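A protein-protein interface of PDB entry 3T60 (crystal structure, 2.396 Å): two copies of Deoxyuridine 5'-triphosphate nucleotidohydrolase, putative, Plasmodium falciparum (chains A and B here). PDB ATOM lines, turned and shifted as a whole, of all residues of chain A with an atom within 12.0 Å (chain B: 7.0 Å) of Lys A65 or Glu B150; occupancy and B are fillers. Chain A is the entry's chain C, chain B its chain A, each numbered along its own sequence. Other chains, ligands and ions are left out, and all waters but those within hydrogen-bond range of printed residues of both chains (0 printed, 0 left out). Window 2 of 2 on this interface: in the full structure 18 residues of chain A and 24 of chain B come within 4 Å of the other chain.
Among the printed residues, pairs that only touch across the chains: Tyr A64 with Leu B147 (3.6 Å), Tyr A63 with Leu B56 (3.6 Å), Tyr A64 with Ser B148 (3.8 Å) and Lys A65 with His B2 (3.8 Å).
N of Glu B150 lies within hydrogen-bond range of O of Leu B3 (2.9 Å). The backbone carbonyl oxygen (O) of Met B1 sits at hydrogen-bond distance from the backbone NH (N) of Ser B148 (3.0 Å). OG of Ser B148 sits at hydrogen-bond distance from ND1 of His B2, at 2.7 Å. O of His B2 sits at hydrogen-bond distance from N of Leu B56 (2.7 Å). The side-chain carboxylate (OE2) of Glu B150 is in hydrogen-bond range of a ring nitrogen (NE2) of His B2 (2.5 Å). The backbone carbonyl oxygen (O) of Ser B148 is in hydrogen-bond range of the backbone NH (N) of Leu B3 (2.8 Å).
Printed residues of chain B within 4 Å of Tyr A64: Leu B147 (3.6 Å) and Ser B148 (3.8 Å). Lys A65 touches three residues of chain B. Printed residues of chain A within 4 Å of Met B1: Tyr A63 (2.8 Å). No residue of chain A comes within 4 Å of Lys B4. No residue of chain A comes within 4 Å of Ile B5. Of the printed residues of chain A, Leu B56 touches Tyr A63. Of chain A, only Tyr A64 (3.8 Å) and Lys A65 (2.9 Å) come within 4 Å of Ser B148. No residue of chain A comes within 4 Å of Phe B149. Printed residues of chain A within 4 Å of Glu B150: Lys A65. Leu B151 touches none of the printed residues of chain A. No residue of chain A comes within 4 Å of Val B152. The nearest residue of chain B that does not touch Lys A65 is Lys B4 (4.6 Å). The nearest printed residue of chain A that does not touch Leu B147 is Tyr A63 (6.2 Å).
NZ of Lys A65 is in salt-bridge range of OE2 of Glu B150, at 3.2 Å. The backbone carbonyl oxygen (O) of Tyr A63 sits at hydrogen-bond distance from the backbone NH (N) of Met B1 (2.8 Å). The side-chain hydroxyl (OG) of Ser B148 lies within hydrogen-bond range of the backbone NH (N) of Lys A65 (2.9 Å). N of His B2 lies within hydrogen-bond range of O of Tyr A63, 3.4 Å away.
Hydrophobic or aromatic side chains of chain B within 4 Å of the printed part of chain A: His B2. Among the printed residues, 8 pairs touch across the chains.
No position is printed for both chains. Of the 8 pairs that touch across the chains among the printed residues, none has its exchanged pair printed and touching as well.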
ATOM      1  N   ASN A  61     -18.809 -21.000  28.661  1.00  0.00           N
ATOM      2  CA  ASN A  61     -18.336 -21.068  27.254  1.00  0.00           C
ATOM      3  C   ASN A  61     -18.342 -19.634  26.707  1.00  0.00           C
ATOM      4  O   ASN A  61     -19.346 -18.932  26.871  1.00  0.00           O
ATOM      5  N   TYR A  62     -17.244 -19.192  26.092  1.00  0.00           N
ATOM      6  CA  TYR A  62     -17.174 -17.807  25.558  1.00  0.00           C
ATOM      7  C   TYR A  62     -16.557 -17.673  24.145  1.00  0.00           C
ATOM      8  O   TYR A  62     -15.648 -18.450  23.769  1.00  0.00           O
ATOM      9  CB  TYR A  62     -16.487 -16.866  26.569  1.00  0.00           C
ATOM     10  CG  TYR A  62     -15.087 -17.259  26.894  1.00  0.00           C
ATOM     11  CD1 TYR A  62     -14.020 -16.749  26.167  1.00  0.00           C
ATOM     12  CD2 TYR A  62     -14.818 -18.148  27.921  1.00  0.00           C
ATOM     13  CE1 TYR A  62     -12.728 -17.125  26.436  1.00  0.00           C
ATOM     14  CE2 TYR A  62     -13.499 -18.546  28.209  1.00  0.00           C
ATOM     15  CZ  TYR A  62     -12.466 -18.021  27.467  1.00  0.00           C
ATOM     16  OH  TYR A  62     -11.161 -18.375  27.741  1.00  0.00           O
ATOM     17  N   TYR A  63     -17.049 -16.688  23.371  1.00  0.00           N
ATOM     18  CA  TYR A  63     -16.503 -16.439  22.022  1.00  0.00           C
ATOM     19  C   TYR A  63     -15.108 -15.804  21.961  1.00  0.00           C
ATOM     20  O   TYR A  63     -14.920 -14.647  22.260  1.00  0.00           O
ATOM     21  CB  TYR A  63     -17.471 -15.719  21.088  1.00  0.00           C
ATOM     22  CG  TYR A  63     -17.037 -15.842  19.637  1.00  0.00           C
ATOM     23  CD1 TYR A  63     -16.571 -17.071  19.127  1.00  0.00           C
ATOM     24  CD2 TYR A  63     -17.086 -14.752  18.772  1.00  0.00           C
ATOM     25  CE1 TYR A  63     -16.164 -17.201  17.794  1.00  0.00           C
ATOM     26  CE2 TYR A  63     -16.701 -14.872  17.427  1.00  0.00           C
ATOM     27  CZ  TYR A  63     -16.245 -16.099  16.947  1.00  0.00           C
ATOM     28  OH  TYR A  63     -15.829 -16.218  15.629  1.00  0.00           O
ATOM     29  N   TYR A  64     -14.134 -16.601  21.555  1.00  0.00           N
ATOM     30  CA  TYR A  64     -12.750 -16.198  21.545  1.00  0.00           C
ATOM     31  C   TYR A  64     -12.172 -16.683  20.189  1.00  0.00           C
ATOM     32  O   TYR A  64     -12.387 -17.853  19.764  1.00  0.00           O
ATOM     33  CB  TYR A  64     -12.013 -16.787  22.778  1.00  0.00           C
ATOM     34  CG  TYR A  64     -10.643 -16.178  22.988  1.00  0.00           C
ATOM     35  CD1 TYR A  64      -9.512 -16.710  22.353  1.00  0.00           C
ATOM     36  CD2 TYR A  64     -10.481 -15.042  23.770  1.00  0.00           C
ATOM     37  CE1 TYR A  64      -8.251 -16.117  22.493  1.00  0.00           C
ATOM     38  CE2 TYR A  64      -9.222 -14.448  23.932  1.00  0.00           C
ATOM     39  CZ  TYR A  64      -8.116 -14.988  23.297  1.00  0.00           C
ATOM     40  OH  TYR A  64      -6.884 -14.390  23.433  1.00  0.00           O
ATOM     41  N   LYS A  65     -11.464 -15.789  19.493  1.00  0.00           N
ATOM     42  CA  LYS A  65     -11.024 -16.092  18.135  1.00  0.00           C
ATOM     43  C   LYS A  65      -9.702 -15.410  17.769  1.00  0.00           C
ATOM     44  O   LYS A  65      -8.688 -15.619  18.432  1.00  0.00           O
ATOM     45  CB  LYS A  65     -12.129 -15.724  17.146  1.00  0.00           C
ATOM     46  CG  LYS A  65     -11.863 -16.175  15.731  1.00  0.00           C
ATOM     47  CD  LYS A  65     -12.874 -15.561  14.814  1.00  0.00           C
ATOM     48  CE  LYS A  65     -12.213 -15.102  13.547  1.00  0.00           C
ATOM     49  NZ  LYS A  65     -13.294 -14.551  12.680  1.00  0.00           N
ATOM     50  N   MET B   1     -14.884 -12.846  24.437  1.00  0.00           N
ATOM     51  CA  MET B   1     -15.680 -11.981  23.500  1.00  0.00           C
ATOM     52  C   MET B   1     -14.732 -11.537  22.415  1.00  0.00           C
ATOM     53  O   MET B   1     -13.563 -11.289  22.702  1.00  0.00           O
ATOM     54  CB  MET B   1     -16.317 -10.774  24.205  1.00  0.00           C
ATOM     55  CG  MET B   1     -16.338  -9.436  23.347  1.00  0.00           C
ATOM     56  SD  MET B   1     -16.906  -7.978  24.286  1.00  0.00           S
ATOM     57  CE  MET B   1     -15.700  -6.733  23.799  1.00  0.00           C
ATOM     58  N   HIS B   2     -15.238 -11.407  21.177  1.00  0.00           N
ATOM     59  CA  HIS B   2     -14.359 -11.072  20.076  1.00  0.00           C
ATOM     60  C   HIS B   2     -14.659  -9.723  19.452  1.00  0.00           C
ATOM     61  O   HIS B   2     -15.780  -9.397  19.168  1.00  0.00           O
ATOM     62  CB  HIS B   2     -14.355 -12.204  19.053  1.00  0.00           C
ATOM     63  CG  HIS B   2     -13.465 -11.960  17.896  1.00  0.00           C
ATOM     64  ND1 HIS B   2     -12.095 -11.988  17.998  1.00  0.00           N
ATOM     65  CD2 HIS B   2     -13.748 -11.675  16.604  1.00  0.00           C
ATOM     66  CE1 HIS B   2     -11.567 -11.708  16.820  1.00  0.00           C
ATOM     67  NE2 HIS B   2     -12.554 -11.523  15.957  1.00  0.00           N
ATOM     68  N   LEU B   3     -13.645  -8.905  19.245  1.00  0.00           N
ATOM     69  CA  LEU B   3     -13.929  -7.625  18.691  1.00  0.00           C
ATOM     70  C   LEU B   3     -13.402  -7.549  17.256  1.00  0.00           C
ATOM     71  O   LEU B   3     -12.270  -7.967  16.980  1.00  0.00           O
ATOM     72  CB  LEU B   3     -13.268  -6.527  19.520  1.00  0.00           C
ATOM     73  CG  LEU B   3     -13.845  -6.172  20.865  1.00  0.00           C
ATOM     74  CD1 LEU B   3     -12.679  -5.800  21.753  1.00  0.00           C
ATOM     75  CD2 LEU B   3     -14.789  -4.971  20.674  1.00  0.00           C
ATOM     76  N   LYS B   4     -14.207  -6.950  16.379  1.00  0.00           N
ATOM     77  CA  LYS B   4     -13.734  -6.529  15.076  1.00  0.00           C
ATOM     78  C   LYS B   4     -13.578  -5.020  15.075  1.00  0.00           C
ATOM     79  O   LYS B   4     -14.522  -4.288  15.296  1.00  0.00           O
ATOM     80  CB  LYS B   4     -14.736  -6.956  14.028  1.00  0.00           C
ATOM     81  CG  LYS B   4     -15.036  -8.433  14.149  1.00  0.00           C
ATOM     82  CD  LYS B   4     -15.867  -8.950  12.992  1.00  0.00           C
ATOM     83  CE  LYS B   4     -15.390 -10.360  12.650  1.00  0.00           C
ATOM     84  NZ  LYS B   4     -16.289 -11.158  11.789  1.00  0.00           N
ATOM     85  N   ILE B   5     -12.386  -4.557  14.769  1.00  0.00           N
ATOM     86  CA  ILE B   5     -12.049  -3.153  14.827  1.00  0.00           C
ATOM     87  C   ILE B   5     -11.710  -2.646  13.420  1.00  0.00           C
ATOM     88  O   ILE B   5     -10.896  -3.287  12.664  1.00  0.00           O
ATOM     89  CB  ILE B   5     -10.828  -2.929  15.800  1.00  0.00           C
ATOM     90  CG1 ILE B   5     -11.149  -3.441  17.214  1.00  0.00           C
ATOM     91  CG2 ILE B   5     -10.443  -1.491  15.845  1.00  0.00           C
ATOM     92  CD1 ILE B   5      -9.956  -3.441  18.093  1.00  0.00           C
ATOM     93  N   VAL B   6     -12.322  -1.508  13.061  1.00  0.00           N
ATOM     94  CA  VAL B   6     -11.968  -0.820  11.850  1.00  0.00           C
ATOM     95  C   VAL B   6     -11.096   0.360  12.263  1.00  0.00           C
ATOM     96  O   VAL B   6     -11.583   1.240  13.004  1.00  0.00           O
ATOM     97  CB  VAL B   6     -13.231  -0.228  11.147  1.00  0.00           C
ATOM     98  CG1 VAL B   6     -12.841   0.523   9.873  1.00  0.00           C
ATOM     99  CG2 VAL B   6     -14.250  -1.276  10.866  1.00  0.00           C
ATOM    100  N   LEU B  56     -18.476  -9.469  19.505  1.00  0.00           N
ATOM    101  CA  LEU B  56     -19.217 -10.658  19.191  1.00  0.00           C
ATOM    102  C   LEU B  56     -19.050 -11.611  20.332  1.00  0.00           C
ATOM    103  O   LEU B  56     -17.934 -11.864  20.762  1.00  0.00           O
ATOM    104  CB  LEU B  56     -18.791 -11.260  17.820  1.00  0.00           C
ATOM    105  CG  LEU B  56     -18.702 -10.343  16.587  1.00  0.00           C
ATOM    106  CD1 LEU B  56     -17.922 -11.015  15.476  1.00  0.00           C
ATOM    107  CD2 LEU B  56     -20.077  -9.931  16.083  1.00  0.00           C
ATOM    108  N   LEU B 147     -10.638 -11.182  25.980  1.00  0.00           N
ATOM    109  CA  LEU B 147     -10.973 -10.491  24.746  1.00  0.00           C
ATOM    110  C   LEU B 147     -10.019 -10.890  23.645  1.00  0.00           C
ATOM    111  O   LEU B 147      -8.793 -10.868  23.855  1.00  0.00           O
ATOM    112  CB  LEU B 147     -10.876  -8.937  24.891  1.00  0.00           C
ATOM    113  CG  LEU B 147     -11.804  -8.197  25.841  1.00  0.00           C
ATOM    114  CD1 LEU B 147     -11.797  -6.761  25.526  1.00  0.00           C
ATOM    115  CD2 LEU B 147     -13.168  -8.699  25.665  1.00  0.00           C
ATOM    116  N   SER B 148     -10.546 -11.194  22.465  1.00  0.00           N
ATOM    117  CA  SER B 148      -9.684 -11.160  21.288  1.00  0.00           C
ATOM    118  C   SER B 148     -10.140 -10.055  20.345  1.00  0.00           C
ATOM    119  O   SER B 148     -11.207  -9.500  20.508  1.00  0.00           O
ATOM    120  CB  SER B 148      -9.574 -12.537  20.573  1.00  0.00           C
ATOM    121  OG  SER B 148     -10.816 -13.006  20.107  1.00  0.00           O
ATOM    122  N   PHE B 149      -9.320  -9.733  19.362  1.00  0.00           N
ATOM    123  CA  PHE B 149      -9.688  -8.746  18.349  1.00  0.00           C
ATOM    124  C   PHE B 149      -8.983  -9.040  17.002  1.00  0.00           C
ATOM    125  O   PHE B 149      -7.925  -9.737  16.951  1.00  0.00           O
ATOM    126  CB  PHE B 149      -9.376  -7.324  18.828  1.00  0.00           C
ATOM    127  CG  PHE B 149      -7.944  -6.911  18.631  1.00  0.00           C
ATOM    128  CD1 PHE B 149      -7.524  -6.342  17.431  1.00  0.00           C
ATOM    129  CD2 PHE B 149      -6.999  -7.101  19.627  1.00  0.00           C
ATOM    130  CE1 PHE B 149      -6.157  -5.916  17.235  1.00  0.00           C
ATOM    131  CE2 PHE B 149      -5.654  -6.685  19.431  1.00  0.00           C
ATOM    132  CZ  PHE B 149      -5.254  -6.093  18.239  1.00  0.00           C
ATOM    133  N   GLU B 150      -9.564  -8.496  15.935  1.00  0.00           N
ATOM    134  CA  GLU B 150      -8.948  -8.497  14.612  1.00  0.00           C
ATOM    135  C   GLU B 150      -9.272  -7.159  13.914  1.00  0.00           C
ATOM    136  O   GLU B 150     -10.248  -6.494  14.229  1.00  0.00           O
ATOM    137  CB  GLU B 150      -9.433  -9.714  13.789  1.00  0.00           C
ATOM    138  CG  GLU B 150     -10.873  -9.625  13.506  1.00  0.00           C
ATOM    139  CD  GLU B 150     -11.449 -10.849  12.799  1.00  0.00           C
ATOM    140  OE1 GLU B 150     -11.356 -10.949  11.557  1.00  0.00           O
ATOM    141  OE2 GLU B 150     -12.075 -11.688  13.484  1.00  0.00           O
ATOM    142  N   LEU B 151      -8.442  -6.764  12.980  1.00  0.00           N
ATOM    143  CA  LEU B 151      -8.700  -5.607  12.159  1.00  0.00           C
ATOM    144  C   LEU B 151      -9.455  -5.997  10.856  1.00  0.00           C
ATOM    145  O   LEU B 151      -9.188  -7.023  10.202  1.00  0.00           O
ATOM    146  CB  LEU B 151      -7.403  -4.837  11.843  1.00  0.00           C
ATOM    147  CG  LEU B 151      -6.488  -4.593  13.066  1.00  0.00           C
ATOM    148  CD1 LEU B 151      -5.135  -3.892  12.690  1.00  0.00           C
ATOM    149  CD2 LEU B 151      -7.202  -3.821  14.178  1.00  0.00           C
ATOM    150  N   VAL B 152     -10.389  -5.117  10.485  1.00  0.00           N
ATOM    151  CA  VAL B 152     -11.414  -5.415   9.521  1.00  0.00           C
ATOM    152  C   VAL B 152     -11.578  -4.098   8.738  1.00  0.00           C
ATOM    153  O   VAL B 152     -11.142  -3.039   9.192  1.00  0.00           O
ATOM    154  CB  VAL B 152     -12.548  -6.014  10.385  1.00  0.00           C
ATOM    155  CG1 VAL B 152     -13.740  -5.212  10.512  1.00  0.00           C
ATOM    156  CG2 VAL B 152     -12.770  -7.451  10.105  1.00  0.00           C
